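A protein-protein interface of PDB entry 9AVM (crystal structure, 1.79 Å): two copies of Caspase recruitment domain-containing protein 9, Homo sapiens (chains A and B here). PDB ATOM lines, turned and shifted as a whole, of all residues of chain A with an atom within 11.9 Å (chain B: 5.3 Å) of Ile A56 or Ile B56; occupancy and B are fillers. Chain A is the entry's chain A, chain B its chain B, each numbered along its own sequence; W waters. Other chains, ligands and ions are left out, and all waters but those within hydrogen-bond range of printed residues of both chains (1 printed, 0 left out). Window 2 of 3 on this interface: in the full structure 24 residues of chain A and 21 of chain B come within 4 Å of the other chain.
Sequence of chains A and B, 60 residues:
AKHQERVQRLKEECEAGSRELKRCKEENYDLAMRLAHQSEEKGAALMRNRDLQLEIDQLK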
ATOM      1  N   LEU A  46     -22.655   0.899 -12.249  1.00  0.00           N
ATOM      2  CA  LEU A  46     -23.873   1.554 -11.798  1.00  0.00           C
ATOM      3  C   LEU A  46     -25.101   0.774 -12.190  1.00  0.00           C
ATOM      4  O   LEU A  46     -26.061   0.792 -11.431  1.00  0.00           O
ATOM      5  CB  LEU A  46     -23.990   2.985 -12.330  1.00  0.00           C
ATOM      6  CG  LEU A  46     -22.998   3.952 -11.732  1.00  0.00           C
ATOM      7  CD1 LEU A  46     -23.087   5.269 -12.455  1.00  0.00           C
ATOM      8  CD2 LEU A  46     -23.180   4.117 -10.215  1.00  0.00           C
ATOM      9  N   MET A  47     -25.089   0.084 -13.340  1.00  0.00           N
ATOM     10  CA  MET A  47     -26.210  -0.742 -13.759  1.00  0.00           C
ATOM     11  C   MET A  47     -26.347  -1.933 -12.811  1.00  0.00           C
ATOM     12  O   MET A  47     -27.458  -2.258 -12.389  1.00  0.00           O
ATOM     13  CB  MET A  47     -25.994  -1.274 -15.173  1.00  0.00           C
ATOM     14  CG  MET A  47     -27.223  -1.925 -15.734  1.00  0.00           C
ATOM     15  SD  MET A  47     -26.833  -2.866 -17.214  1.00  0.00           S
ATOM     16  CE  MET A  47     -26.372  -4.430 -16.474  1.00  0.00           C
ATOM     17  N   ARG A  48     -25.217  -2.570 -12.457  1.00  0.00           N
ATOM     18  CA  ARG A  48     -25.207  -3.695 -11.517  1.00  0.00           C
ATOM     19  C   ARG A  48     -25.753  -3.231 -10.156  1.00  0.00           C
ATOM     20  O   ARG A  48     -26.553  -3.934  -9.545  1.00  0.00           O
ATOM     21  CB  ARG A  48     -23.783  -4.292 -11.412  1.00  0.00           C
ATOM     22  CG  ARG A  48     -23.654  -5.487 -10.463  1.00  0.00           C
ATOM     23  CD  ARG A  48     -24.480  -6.685 -10.916  1.00  0.00           C
ATOM     24  NE  ARG A  48     -24.335  -7.845 -10.022  1.00  0.00           N
ATOM     25  CZ  ARG A  48     -25.311  -8.712  -9.763  1.00  0.00           C
ATOM     26  NH1 ARG A  48     -26.519  -8.546 -10.297  1.00  0.00           N
ATOM     27  NH2 ARG A  48     -25.097  -9.740  -8.948  1.00  0.00           N
ATOM     28  N   ASN A  49     -25.376  -2.024  -9.720  1.00  0.00           N
ATOM     29  CA  ASN A  49     -25.845  -1.425  -8.473  1.00  0.00           C
ATOM     30  C   ASN A  49     -27.359  -1.238  -8.457  1.00  0.00           C
ATOM     31  O   ASN A  49     -27.995  -1.527  -7.444  1.00  0.00           O
ATOM     32  CB  ASN A  49     -25.145  -0.081  -8.243  1.00  0.00           C
ATOM     33  CG  ASN A  49     -25.480   0.602  -6.946  1.00  0.00           C
ATOM     34  OD1 ASN A  49     -26.403   1.414  -6.874  1.00  0.00           O
ATOM     35  ND2 ASN A  49     -24.758   0.272  -5.879  1.00  0.00           N
ATOM     36  N   ARG A  50     -27.929  -0.755  -9.566  1.00  0.00           N
ATOM     37  CA  ARG A  50     -29.376  -0.556  -9.672  1.00  0.00           C
ATOM     38  C   ARG A  50     -30.107  -1.887  -9.546  1.00  0.00           C
ATOM     39  O   ARG A  50     -31.070  -1.970  -8.786  1.00  0.00           O
ATOM     40  CB  ARG A  50     -29.739   0.142 -10.988  1.00  0.00           C
ATOM     41  CG  ARG A  50     -29.309   1.610 -10.965  1.00  0.00           C
ATOM     42  CD  ARG A  50     -29.894   2.413 -12.117  1.00  0.00           C
ATOM     43  NE  ARG A  50     -29.518   1.884 -13.429  1.00  0.00           N
ATOM     44  CZ  ARG A  50     -28.471   2.311 -14.139  1.00  0.00           C
ATOM     45  NH1 ARG A  50     -27.707   3.297 -13.685  1.00  0.00           N
ATOM     46  NH2 ARG A  50     -28.218   1.798 -15.333  1.00  0.00           N
ATOM     47  N   ASP A  51     -29.612  -2.935 -10.218  1.00  0.00           N
ATOM     48  CA  ASP A  51     -30.203  -4.273 -10.174  1.00  0.00           C
ATOM     49  C   ASP A  51     -30.159  -4.869  -8.768  1.00  0.00           C
ATOM     50  O   ASP A  51     -31.142  -5.468  -8.330  1.00  0.00           O
ATOM     51  CB  ASP A  51     -29.505  -5.214 -11.156  1.00  0.00           C
ATOM     52  CG  ASP A  51     -29.731  -4.880 -12.618  1.00  0.00           C
ATOM     53  OD1 ASP A  51     -30.658  -4.086 -12.913  1.00  0.00           O
ATOM     54  OD2 ASP A  51     -28.973  -5.401 -13.465  1.00  0.00           O
ATOM     55  N   LEU A  52     -29.026  -4.700  -8.068  1.00  0.00           N
ATOM     56  CA  LEU A  52     -28.877  -5.190  -6.690  1.00  0.00           C
ATOM     57  C   LEU A  52     -29.808  -4.443  -5.741  1.00  0.00           C
ATOM     58  O   LEU A  52     -30.425  -5.066  -4.879  1.00  0.00           O
ATOM     59  CB  LEU A  52     -27.416  -5.049  -6.214  1.00  0.00           C
ATOM     60  CG  LEU A  52     -26.414  -5.954  -6.930  1.00  0.00           C
ATOM     61  CD1 LEU A  52     -24.981  -5.604  -6.554  1.00  0.00           C
ATOM     62  CD2 LEU A  52     -26.702  -7.425  -6.657  1.00  0.00           C
ATOM     63  N   GLN A  53     -29.935  -3.119  -5.908  1.00  0.00           N
ATOM     64  CA  GLN A  53     -30.822  -2.331  -5.056  1.00  0.00           C
ATOM     65  C   GLN A  53     -32.279  -2.765  -5.232  1.00  0.00           C
ATOM     66  O   GLN A  53     -33.022  -2.839  -4.253  1.00  0.00           O
ATOM     67  CB  GLN A  53     -30.669  -0.828  -5.325  1.00  0.00           C
ATOM     68  CG  GLN A  53     -31.407   0.056  -4.323  1.00  0.00           C
ATOM     69  CD  GLN A  53     -30.978  -0.191  -2.895  1.00  0.00           C
ATOM     70  OE1 GLN A  53     -29.823   0.031  -2.519  1.00  0.00           O
ATOM     71  NE2 GLN A  53     -31.905  -0.654  -2.061  1.00  0.00           N
ATOM     72  N   LEU A  54     -32.674  -3.086  -6.459  1.00  0.00           N
ATOM     73  CA  LEU A  54     -34.018  -3.570  -6.759  1.00  0.00           C
ATOM     74  C   LEU A  54     -34.276  -4.909  -6.060  1.00  0.00           C
ATOM     75  O   LEU A  54     -35.380  -5.116  -5.579  1.00  0.00           O
ATOM     76  CB  LEU A  54     -34.169  -3.743  -8.284  1.00  0.00           C
ATOM     77  CG  LEU A  54     -34.937  -2.679  -9.091  1.00  0.00           C
ATOM     78  CD1 LEU A  54     -34.825  -1.253  -8.495  1.00  0.00           C
ATOM     79  CD2 LEU A  54     -34.495  -2.686 -10.530  1.00  0.00           C
ATOM     80  N   GLU A  55     -33.273  -5.813  -6.016  1.00  0.00           N
ATOM     81  CA  GLU A  55     -33.374  -7.122  -5.361  1.00  0.00           C
ATOM     82  C   GLU A  55     -33.607  -6.958  -3.863  1.00  0.00           C
ATOM     83  O   GLU A  55     -34.474  -7.633  -3.305  1.00  0.00           O
ATOM     84  CB  GLU A  55     -32.087  -7.940  -5.578  1.00  0.00           C
ATOM     85  CG  GLU A  55     -31.963  -8.587  -6.937  1.00  0.00           C
ATOM     86  CD  GLU A  55     -30.750  -9.489  -7.065  1.00  0.00           C
ATOM     87  OE1 GLU A  55     -30.530 -10.322  -6.155  1.00  0.00           O
ATOM     88  OE2 GLU A  55     -30.025  -9.371  -8.080  1.00  0.00           O
ATOM     89  N   ILE A  56     -32.820  -6.076  -3.214  1.00  0.00           N
ATOM     90  CA  ILE A  56     -32.901  -5.778  -1.784  1.00  0.00           C
ATOM     91  C   ILE A  56     -34.272  -5.226  -1.398  1.00  0.00           C
ATOM     92  O   ILE A  56     -34.841  -5.643  -0.384  1.00  0.00           O
ATOM     93  CB  ILE A  56     -31.780  -4.783  -1.412  1.00  0.00           C
ATOM     94  CG1 ILE A  56     -30.446  -5.489  -1.458  1.00  0.00           C
ATOM     95  CG2 ILE A  56     -32.005  -4.137  -0.039  1.00  0.00           C
ATOM     96  CD1 ILE A  56     -29.333  -4.643  -1.446  1.00  0.00           C
ATOM     97  N   ASP A  57     -34.786  -4.282  -2.196  1.00  0.00           N
ATOM     98  CA  ASP A  57     -36.078  -3.651  -1.950  1.00  0.00           C
ATOM     99  C   ASP A  57     -37.237  -4.661  -1.964  1.00  0.00           C
ATOM    100  O   ASP A  57     -38.225  -4.463  -1.257  1.00  0.00           O
ATOM    101  CB  ASP A  57     -36.319  -2.529  -2.973  1.00  0.00           C
ATOM    102  CG  ASP A  57     -35.455  -1.298  -2.792  1.00  0.00           C
ATOM    103  OD1 ASP A  57     -35.455  -0.433  -3.701  1.00  0.00           O
ATOM    104  OD2 ASP A  57     -34.774  -1.196  -1.748  1.00  0.00           O
ATOM    105  N   GLN A  58     -37.102  -5.749  -2.735  1.00  0.00           N
ATOM    106  CA  GLN A  58     -38.104  -6.807  -2.807  1.00  0.00           C
ATOM    107  C   GLN A  58     -38.042  -7.751  -1.595  1.00  0.00           C
ATOM    108  O   GLN A  58     -39.058  -8.343  -1.236  1.00  0.00           O
ATOM    109  CB  GLN A  58     -37.940  -7.609  -4.107  1.00  0.00           C
ATOM    110  CG  GLN A  58     -38.244  -6.788  -5.362  1.00  0.00           C
ATOM    111  CD  GLN A  58     -37.713  -7.387  -6.657  1.00  0.00           C
ATOM    112  OE1 GLN A  58     -37.820  -6.773  -7.730  1.00  0.00           O
ATOM    113  NE2 GLN A  58     -37.111  -8.583  -6.605  1.00  0.00           N
ATOM    114  N   LEU A  59     -36.867  -7.898  -0.973  1.00  0.00           N
ATOM    115  CA  LEU A  59     -36.704  -8.781   0.177  1.00  0.00           C
ATOM    116  C   LEU A  59     -36.985  -8.079   1.506  1.00  0.00           C
ATOM    117  O   LEU A  59     -37.527  -8.692   2.420  1.00  0.00           O
ATOM    118  CB  LEU A  59     -35.296  -9.374   0.200  1.00  0.00           C
ATOM    119  CG  LEU A  59     -34.894 -10.171  -1.020  1.00  0.00           C
ATOM    120  CD1 LEU A  59     -33.401 -10.511  -0.994  1.00  0.00           C
ATOM    121  CD2 LEU A  59     -35.732 -11.411  -1.143  1.00  0.00           C
ATOM    122  N   LYS A  60     -36.583  -6.806   1.620  1.00  0.00           N
ATOM    123  CA  LYS A  60     -36.772  -6.019   2.836  1.00  0.00           C
ATOM    124  C   LYS A  60     -38.167  -5.414   2.896  1.00  0.00           C
ATOM    125  O   LYS A  60     -38.607  -4.772   1.940  1.00  0.00           O
ATOM    126  CB  LYS A  60     -35.707  -4.916   2.936  1.00  0.00           C
ATOM    127  CG  LYS A  60     -34.370  -5.435   3.423  1.00  0.00           C
ATOM    128  CD  LYS A  60     -33.267  -4.381   3.432  1.00  0.00           C
ATOM    129  CE  LYS A  60     -33.542  -3.225   4.352  1.00  0.00           C
ATOM    130  NZ  LYS A  60     -32.287  -2.564   4.800  1.00  0.00           N
ATOM    131  N   LEU B  52     -24.143  -4.660  -0.942  1.00  0.00           N
ATOM    132  CA  LEU B  52     -25.516  -5.018  -1.274  1.00  0.00           C
ATOM    133  C   LEU B  52     -25.642  -6.522  -1.463  1.00  0.00           C
ATOM    134  O   LEU B  52     -26.619  -7.107  -0.984  1.00  0.00           O
ATOM    135  CB  LEU B  52     -25.994  -4.291  -2.544  1.00  0.00           C
ATOM    136  CG  LEU B  52     -26.171  -2.774  -2.424  1.00  0.00           C
ATOM    137  CD1 LEU B  52     -26.558  -2.166  -3.756  1.00  0.00           C
ATOM    138  CD2 LEU B  52     -27.191  -2.402  -1.390  1.00  0.00           C
ATOM    139  N   GLN B  53     -24.650  -7.165  -2.122  1.00  0.00           N
ATOM    140  CA  GLN B  53     -24.698  -8.607  -2.316  1.00  0.00           C
ATOM    141  C   GLN B  53     -24.668  -9.346  -0.979  1.00  0.00           C
ATOM    142  O   GLN B  53     -25.389 -10.325  -0.798  1.00  0.00           O
ATOM    143  CB  GLN B  53     -23.570  -9.086  -3.232  1.00  0.00           C
ATOM    144  CG  GLN B  53     -23.704 -10.563  -3.626  1.00  0.00           C
ATOM    145  CD  GLN B  53     -25.000 -10.887  -4.338  1.00  0.00           C
ATOM    146  OE1 GLN B  53     -25.268 -10.397  -5.428  1.00  0.00           O
ATOM    147  NE2 GLN B  53     -25.833 -11.741  -3.740  1.00  0.00           N
ATOM    148  N   LEU B  54     -23.863  -8.859  -0.045  1.00  0.00           N
ATOM    149  CA  LEU B  54     -23.784  -9.438   1.297  1.00  0.00           C
ATOM    150  C   LEU B  54     -25.141  -9.341   2.034  1.00  0.00           C
ATOM    151  O   LEU B  54     -25.525 -10.281   2.734  1.00  0.00           O
ATOM    152  CB  LEU B  54     -22.708  -8.697   2.088  1.00  0.00           C
ATOM    153  CG  LEU B  54     -21.322  -9.334   2.267  1.00  0.00           C
ATOM    154  CD1 LEU B  54     -20.891 -10.227   1.083  1.00  0.00           C
ATOM    155  CD2 LEU B  54     -20.274  -8.262   2.527  1.00  0.00           C
ATOM    156  N   GLU B  55     -25.852  -8.208   1.874  1.00  0.00           N
ATOM    157  CA  GLU B  55     -27.163  -7.980   2.484  1.00  0.00           C
ATOM    158  C   GLU B  55     -28.181  -8.960   1.935  1.00  0.00           C
ATOM    159  O   GLU B  55     -28.953  -9.523   2.710  1.00  0.00           O
ATOM    160  CB  GLU B  55     -27.652  -6.548   2.204  1.00  0.00           C
ATOM    161  CG  GLU B  55     -27.017  -5.464   3.053  1.00  0.00           C
ATOM    162  CD  GLU B  55     -27.655  -4.105   2.827  1.00  0.00           C
ATOM    163  OE1 GLU B  55     -28.905  -4.020   2.844  1.00  0.00           O
ATOM    164  OE2 GLU B  55     -26.905  -3.122   2.625  1.00  0.00           O
ATOM    165  N   ILE B  56     -28.203  -9.145   0.588  1.00  0.00           N
ATOM    166  CA  ILE B  56     -29.115 -10.044  -0.113  1.00  0.00           C
ATOM    167  C   ILE B  56     -28.951 -11.487   0.349  1.00  0.00           C
ATOM    168  O   ILE B  56     -29.947 -12.176   0.573  1.00  0.00           O
ATOM    169  CB  ILE B  56     -28.894  -9.920  -1.637  1.00  0.00           C
ATOM    170  CG1 ILE B  56     -29.435  -8.581  -2.121  1.00  0.00           C
ATOM    171  CG2 ILE B  56     -29.540 -11.076  -2.418  1.00  0.00           C
ATOM    172  CD1 ILE B  56     -29.000  -8.241  -3.508  1.00  0.00           C
ATOM    173  N   ASP B  57     -27.700 -11.931   0.474  1.00  0.00           N
ATOM    174  CA  ASP B  57     -27.370 -13.290   0.886  1.00  0.00           C
ATOM    175  C   ASP B  57     -27.930 -13.612   2.286  1.00  0.00           C
ATOM    176  O   ASP B  57     -28.263 -14.760   2.563  1.00  0.00           O
ATOM    177  CB  ASP B  57     -25.845 -13.499   0.821  1.00  0.00           C
ATOM    178  CG  ASP B  57     -25.280 -13.560  -0.587  1.00  0.00           C
ATOM    179  OD1 ASP B  57     -24.043 -13.516  -0.728  1.00  0.00           O
ATOM    180  OD2 ASP B  57     -26.079 -13.654  -1.548  1.00  0.00           O
ATOM    181  N   GLN B  58     -28.060 -12.603   3.151  1.00  0.00           N
ATOM    182  CA  GLN B  58     -28.606 -12.780   4.500  1.00  0.00           C
ATOM    183  C   GLN B  58     -30.155 -12.842   4.493  1.00  0.00           C
ATOM    184  O   GLN B  58     -30.760 -13.469   5.366  1.00  0.00           O
ATOM    185  CB  GLN B  58     -28.102 -11.647   5.423  1.00  0.00           C
ATOM    186  CG  GLN B  58     -26.591 -11.669   5.645  1.00  0.00           C
ATOM    187  CD  GLN B  58     -25.964 -10.369   6.129  1.00  0.00           C
ATOM    188  OE1 GLN B  58     -24.730 -10.258   6.238  1.00  0.00           O
ATOM    189  NE2 GLN B  58     -26.773  -9.347   6.421  1.00  0.00           N
ATOM    190  N   LEU B  59     -30.796 -12.213   3.506  1.00  0.00           N
ATOM    191  CA  LEU B  59     -32.251 -12.155   3.441  1.00  0.00           C
ATOM    192  C   LEU B  59     -32.921 -13.304   2.693  1.00  0.00           C
ATOM    193  O   LEU B  59     -34.072 -13.624   3.023  1.00  0.00           O
ATOM    194  CB  LEU B  59     -32.713 -10.824   2.824  1.00  0.00           C
ATOM    195  CG  LEU B  59     -32.266  -9.557   3.512  1.00  0.00           C
ATOM    196  CD1 LEU B  59     -32.615  -8.342   2.667  1.00  0.00           C
ATOM    197  CD2 LEU B  59     -32.847  -9.453   4.917  1.00  0.00           C
ATOM    198  N   LYS B  60     -32.301 -13.842   1.630  1.00  0.00           N
ATOM    199  CA  LYS B  60     -32.960 -14.884   0.833  1.00  0.00           C
ATOM    200  C   LYS B  60     -32.954 -16.252   1.527  1.00  0.00           C
ATOM    201  O   LYS B  60     -32.078 -16.514   2.346  1.00  0.00           O
ATOM    202  CB  LYS B  60     -32.397 -14.952  -0.606  1.00  0.00           C
ATOM    203  CG  LYS B  60     -31.244 -15.932  -0.841  1.00  0.00           C
ATOM    204  CD  LYS B  60     -29.907 -15.404  -0.346  1.00  0.00           C
ATOM    205  CE  LYS B  60     -28.921 -16.526  -0.112  1.00  0.00           C
ATOM    206  NZ  LYS B  60     -29.183 -17.221   1.177  1.00  0.00           N
HETATM  207  O   HOH W   1     -27.593 -11.012  -7.538  1.00  0.00           O
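Hydrophobic or aromatic side chains of chain A that line the printed part of chain B: Leu A52, Ile A56 and Leu A59.
Of the 9 printed residues of chain B, 4 touch a printed residue of chain A.
Printed residues of chain B that touch a printed residue of chain A: Leu B52, Gln B53, Ile B56 and Leu B59.
Hydrophobic or aromatic side chains of chain B that line the printed part of chain A: Leu B52, Ile B56 and Leu B59.
Among the printed residues, 11 pairs touch across the chains.
Water W1 lies within hydrogen-bond range of OE2 of Glu A55 (3.0 Å), NH2 of Arg A48 (3.1 Å) and OE1 of Gln B53 (3.2 Å).
Arg A48 touches Gln B53 (NH2 to OE1, 3.6 Å).
Asn A49 touches Leu B52.
Leu A52 touches Leu B52 (CB to CD1, 3.9 Å).
Gln B53 touches Leu A52.
Ile B56 touches Leu A52 (CD1 to O, 3.7 Å).
Gln A53 touches Leu B52 (OE1 to CD2, 3.8 Å).
Glu A55 touches Ile B56.
CD2 of Leu B52 touches CD1 of Ile A56 (3.1 Å).
Ile A56 touches Ile B56 (CG1 to CG1, 3.3 Å).
CD1 of Leu B59 touches CB of Leu A59, at 3.8 Å.
The side-chain carboxylate (OD2) of Asp A57 is in hydrogen-bond range of the side-chain amide nitrogen (NE2) of Gln A53, 2.9 Å away.
OD2 of Asp B57 is in hydrogen-bond range of NE2 of Gln B53, 2.9 Å away.
Leu A52 touches Ile B56, and with the chains exchanged Ile A56 touches Leu B52.
Glu A55 touches Ile B56, but with the chains exchanged Ile A56 does not touch Glu B55 (4.2 Å).
Ile B56 touches its own counterpart, Ile A56.
Leu A59 touches its own counterpart, Leu B59.
Positions printed for both chains: 52, 53, 54, 55, 56, 57, 58, 59 and 60.
Printed residues of chain B within 4 Å of Arg A48: Gln B53.
Printed residues of chain B within 4 Å of Asn A49: Leu B52 (3.7 Å).
Printed residues of chain B within 4 Å of Gln A53: Leu B52 (3.8 Å).
Ile A56 touches two residues of chain B.
Printed residues of chain B within 4 Å of Leu A59: Leu B59 (3.8 Å).
Printed residues of chain B within 4 Å of Lys A60: Leu B59.
Leu B52 touches just these residues of chain A: Asn A49, Leu A52, Gln A53 and Ile A56.
Gln B53 touches just these residues of chain A: Arg A48 (3.6 Å) and Leu A52 (3.5 Å).
No residue of chain A comes within 4 Å of Glu B55.
No residue of chain A comes within 4 Å of Asp B57.
Gln B58 touches none of the printed residues of chain A.
Of chain A, only Leu A59 and Lys A60 come within 4 Å of Leu B59.
No residue of chain A comes within 4 Å of Lys B60.
The nearest residue of chain A that does not touch Ile B56 is Leu A59 (4.1 Å).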
